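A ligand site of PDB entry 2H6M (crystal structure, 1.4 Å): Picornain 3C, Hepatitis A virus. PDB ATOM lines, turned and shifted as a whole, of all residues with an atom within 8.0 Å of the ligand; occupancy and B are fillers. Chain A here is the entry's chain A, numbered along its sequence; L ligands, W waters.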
ATOM      1  N   GLU A   4      -0.733 -33.747 -27.157  1.00  0.00           N
ATOM      2  CA  GLU A   4      -1.660 -32.876 -26.431  1.00  0.00           C
ATOM      3  C   GLU A   4      -1.125 -31.453 -26.288  1.00  0.00           C
ATOM      4  O   GLU A   4      -1.875 -30.486 -26.469  1.00  0.00           O
ATOM      5  CB  GLU A   4      -2.064 -33.479 -25.080  1.00  0.00           C
ATOM      6  CG  GLU A   4      -2.904 -34.757 -25.179  1.00  0.00           C
ATOM      7  CD  GLU A   4      -4.285 -34.559 -25.803  1.00  0.00           C
ATOM      8  OE1 GLU A   4      -4.868 -33.463 -25.710  1.00  0.00           O
ATOM      9  OE2 GLU A   4      -4.811 -35.543 -26.363  1.00  0.00           O
ATOM     10  N   ILE A   5       0.186 -31.317 -26.028  1.00  0.00           N
ATOM     11  CA  ILE A   5       0.807 -29.976 -26.070  1.00  0.00           C
ATOM     12  C   ILE A   5       0.643 -29.396 -27.459  1.00  0.00           C
ATOM     13  O   ILE A   5       0.317 -28.213 -27.615  1.00  0.00           O
ATOM     14  CB  ILE A   5       2.307 -29.998 -25.689  1.00  0.00           C
ATOM     15  CG1 ILE A   5       2.482 -30.364 -24.198  1.00  0.00           C
ATOM     16  CG2 ILE A   5       2.976 -28.644 -26.023  1.00  0.00           C
ATOM     17  CD1 ILE A   5       1.938 -29.318 -23.206  1.00  0.00           C
ATOM     18  N   LEU A   8      -2.696 -27.769 -27.962  1.00  0.00           N
ATOM     19  CA  LEU A   8      -2.775 -26.453 -27.296  1.00  0.00           C
ATOM     20  C   LEU A   8      -2.040 -25.383 -28.065  1.00  0.00           C
ATOM     21  O   LEU A   8      -2.508 -24.242 -28.145  1.00  0.00           O
ATOM     22  CB  LEU A   8      -2.208 -26.527 -25.877  1.00  0.00           C
ATOM     23  CG  LEU A   8      -2.881 -27.515 -24.930  1.00  0.00           C
ATOM     24  CD1 LEU A   8      -2.121 -27.516 -23.639  1.00  0.00           C
ATOM     25  CD2 LEU A   8      -4.325 -27.147 -24.709  1.00  0.00           C
ATOM     26  N   ARG A  97      -6.232 -18.703 -24.652  1.00  0.00           N
ATOM     27  CA  ARG A  97      -5.961 -19.609 -23.551  1.00  0.00           C
ATOM     28  C   ARG A  97      -4.526 -19.381 -23.075  1.00  0.00           C
ATOM     29  O   ARG A  97      -3.598 -19.293 -23.881  1.00  0.00           O
ATOM     30  CB  ARG A  97      -6.115 -21.057 -24.019  1.00  0.00           C
ATOM     31  CG  ARG A  97      -5.782 -22.079 -22.951  1.00  0.00           C
ATOM     32  CD  ARG A  97      -6.066 -23.466 -23.464  1.00  0.00           C
ATOM     33  NE  ARG A  97      -5.845 -24.474 -22.431  1.00  0.00           N
ATOM     34  CZ  ARG A  97      -6.389 -25.680 -22.442  1.00  0.00           C
ATOM     35  NH1 ARG A  97      -7.207 -26.047 -23.424  1.00  0.00           N
ATOM     36  NH2 ARG A  97      -6.121 -26.532 -21.460  1.00  0.00           N
ATOM     37  N   ASP A  98      -4.354 -19.255 -21.759  1.00  0.00           N
ATOM     38  CA  ASP A  98      -3.040 -19.062 -21.148  1.00  0.00           C
ATOM     39  C   ASP A  98      -2.268 -20.355 -21.232  1.00  0.00           C
ATOM     40  O   ASP A  98      -2.600 -21.342 -20.547  1.00  0.00           O
ATOM     41  CB  ASP A  98      -3.205 -18.635 -19.677  1.00  0.00           C
ATOM     42  CG  ASP A  98      -1.871 -18.342 -18.986  1.00  0.00           C
ATOM     43  OD1 ASP A  98      -0.797 -18.579 -19.581  1.00  0.00           O
ATOM     44  OD2 ASP A  98      -1.913 -17.874 -17.829  1.00  0.00           O
ATOM     45  N   ILE A  99      -1.250 -20.372 -22.093  1.00  0.00           N
ATOM     46  CA  ILE A  99      -0.366 -21.539 -22.229  1.00  0.00           C
ATOM     47  C   ILE A  99       1.040 -21.312 -21.672  1.00  0.00           C
ATOM     48  O   ILE A  99       1.940 -22.120 -21.905  1.00  0.00           O
ATOM     49  CB  ILE A  99      -0.315 -22.092 -23.687  1.00  0.00           C
ATOM     50  CG1 ILE A  99       0.222 -21.024 -24.669  1.00  0.00           C
ATOM     51  CG2 ILE A  99      -1.684 -22.617 -24.129  1.00  0.00           C
ATOM     52  CD1 ILE A  99       0.545 -21.556 -26.048  1.00  0.00           C
ATOM     53  N   THR A 100       1.223 -20.211 -20.928  1.00  0.00           N
ATOM     54  CA  THR A 100       2.554 -19.872 -20.426  1.00  0.00           C
ATOM     55  C   THR A 100       3.142 -20.937 -19.499  1.00  0.00           C
ATOM     56  O   THR A 100       4.357 -21.148 -19.479  1.00  0.00           O
ATOM     57  CB  THR A 100       2.569 -18.513 -19.693  1.00  0.00           C
ATOM     58  OG1 THR A 100       1.670 -18.565 -18.577  1.00  0.00           O
ATOM     59  CG2 THR A 100       2.165 -17.370 -20.637  1.00  0.00           C
ATOM     60  N   GLN A 101       2.289 -21.655 -18.762  1.00  0.00           N
ATOM     61  CA  GLN A 101       2.785 -22.668 -17.810  1.00  0.00           C
ATOM     62  C   GLN A 101       3.283 -23.940 -18.493  1.00  0.00           C
ATOM     63  O   GLN A 101       3.859 -24.822 -17.834  1.00  0.00           O
ATOM     64  CB  GLN A 101       1.733 -23.008 -16.751  1.00  0.00           C
ATOM     65  CG  GLN A 101       1.274 -21.801 -15.941  1.00  0.00           C
ATOM     66  CD  GLN A 101       2.432 -21.004 -15.378  1.00  0.00           C
ATOM     67  OE1 GLN A 101       2.700 -19.876 -15.818  1.00  0.00           O
ATOM     68  NE2 GLN A 101       3.139 -21.570 -14.411  1.00  0.00           N
ATOM     69  N   HIS A 102       3.072 -24.016 -19.806  1.00  0.00           N
ATOM     70  CA  HIS A 102       3.537 -25.148 -20.606  1.00  0.00           C
ATOM     71  C   HIS A 102       4.900 -24.887 -21.218  1.00  0.00           C
ATOM     72  O   HIS A 102       5.466 -25.784 -21.860  1.00  0.00           O
ATOM     73  CB  HIS A 102       2.510 -25.534 -21.681  1.00  0.00           C
ATOM     74  CG  HIS A 102       1.256 -26.127 -21.106  1.00  0.00           C
ATOM     75  ND1 HIS A 102       1.254 -27.355 -20.468  1.00  0.00           N
ATOM     76  CD2 HIS A 102      -0.016 -25.662 -21.032  1.00  0.00           C
ATOM     77  CE1 HIS A 102       0.036 -27.623 -20.042  1.00  0.00           C
ATOM     78  NE2 HIS A 102      -0.764 -26.617 -20.371  1.00  0.00           N
ATOM     79  N   GLN A 184       6.943 -32.711 -18.953  1.00  0.00           N
ATOM     80  CA  GLN A 184       5.597 -32.513 -19.478  1.00  0.00           C
ATOM     81  C   GLN A 184       5.651 -31.949 -20.896  1.00  0.00           C
ATOM     82  O   GLN A 184       4.862 -31.066 -21.267  1.00  0.00           O
ATOM     83  CB  GLN A 184       4.767 -31.622 -18.546  1.00  0.00           C
ATOM     84  CG  GLN A 184       4.479 -32.279 -17.180  1.00  0.00           C
ATOM     85  CD  GLN A 184       5.693 -32.279 -16.257  1.00  0.00           C
ATOM     86  OE1 GLN A 184       6.291 -31.230 -16.000  1.00  0.00           O
ATOM     87  NE2 GLN A 184       6.060 -33.455 -15.782  1.00  0.00           N
ATOM     88  N   GLN A 206       9.509 -19.872 -19.300  1.00  0.00           N
ATOM     89  CA  GLN A 206       8.452 -19.337 -18.462  1.00  0.00           C
ATOM     90  C   GLN A 206       8.794 -17.984 -17.862  1.00  0.00           C
ATOM     91  O   GLN A 206       7.955 -17.097 -17.800  1.00  0.00           O
ATOM     92  CB  GLN A 206       8.163 -20.276 -17.299  1.00  0.00           C
ATOM     93  CG  GLN A 206       6.992 -21.181 -17.542  1.00  0.00           C
ATOM     94  CD  GLN A 206       6.712 -22.149 -16.409  1.00  0.00           C
ATOM     95  OE1 GLN A 206       6.443 -23.314 -16.640  1.00  0.00           O
ATOM     96  NE2 GLN A 206       6.771 -21.658 -15.166  1.00  0.00           N
HETATM   97  O1  LIG L   1      -4.707 -25.289 -19.662  1.00  0.00           O
HETATM   98  C1  LIG L   1      -4.020 -25.713 -18.702  1.00  0.00           C
HETATM   99  O2  LIG L   1      -4.542 -26.013 -17.594  1.00  0.00           O
HETATM  100  C2  LIG L   1      -2.524 -25.840 -18.903  1.00  0.00           C
HETATM  101  C3  LIG L   1      -2.117 -26.620 -20.167  1.00  0.00           C
HETATM  102  N1  LIG L   1      -1.881 -26.444 -17.753  1.00  0.00           N
HETATM  103  C4  LIG L   1      -1.444 -25.726 -16.722  1.00  0.00           C
HETATM  104  O3  LIG L   1      -1.500 -24.504 -16.658  1.00  0.00           O
HETATM  105  O4  LIG L   1      -0.876 -26.484 -15.631  1.00  0.00           O
HETATM  106  C5  LIG L   1      -0.701 -25.898 -14.351  1.00  0.00           C
HETATM  107  C6  LIG L   1      -0.792 -26.987 -13.317  1.00  0.00           C
HETATM  108  C7  LIG L   1      -0.272 -26.767 -12.045  1.00  0.00           C
HETATM  109  C8  LIG L   1      -0.333 -27.769 -11.071  1.00  0.00           C
HETATM  110  C9  LIG L   1      -0.936 -28.988 -11.380  1.00  0.00           C
HETATM  111  C10 LIG L   1      -1.452 -29.218 -12.652  1.00  0.00           C
HETATM  112  C11 LIG L   1      -1.391 -28.216 -13.626  1.00  0.00           C
HETATM  113  O   HOH W   1      -7.307 -25.807 -18.483  1.00  0.00           O
HETATM  114  O   HOH W   2      -3.321 -23.752 -21.313  1.00  0.00           O
HETATM  115  O   HOH W   3      -0.647 -22.235 -18.682  1.00  0.00           O
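NE2 of His 102 is covalently linked to C3 of the ligand.
O1 of the ligand sits close to NH2 of Arg 97 (2.6 Å).
OE1 of Gln 101 lies within hydrogen-bond range of OG1 of Thr 100.
The backbone carbonyl oxygen (O) of Gln 101 lies close to the side-chain amide oxygen (OE1) of Gln 206 (3.2 Å).
Leu 8 touches the ligand (CD1 to C3, 3.6 Å).
CB of Gln 101 touches O3 of the ligand (3.6 Å).
Hydrophobic or aromatic side chains that line the ligand: Leu 8 and His 102.
Of the 11 residues printed, 4 come within 4 Å of the ligand.
The nearest printed residue that does not touch the ligand is Asp 98 (4.6 Å).
Water W2 bridges O of Asp 98 and NE of Arg 97.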
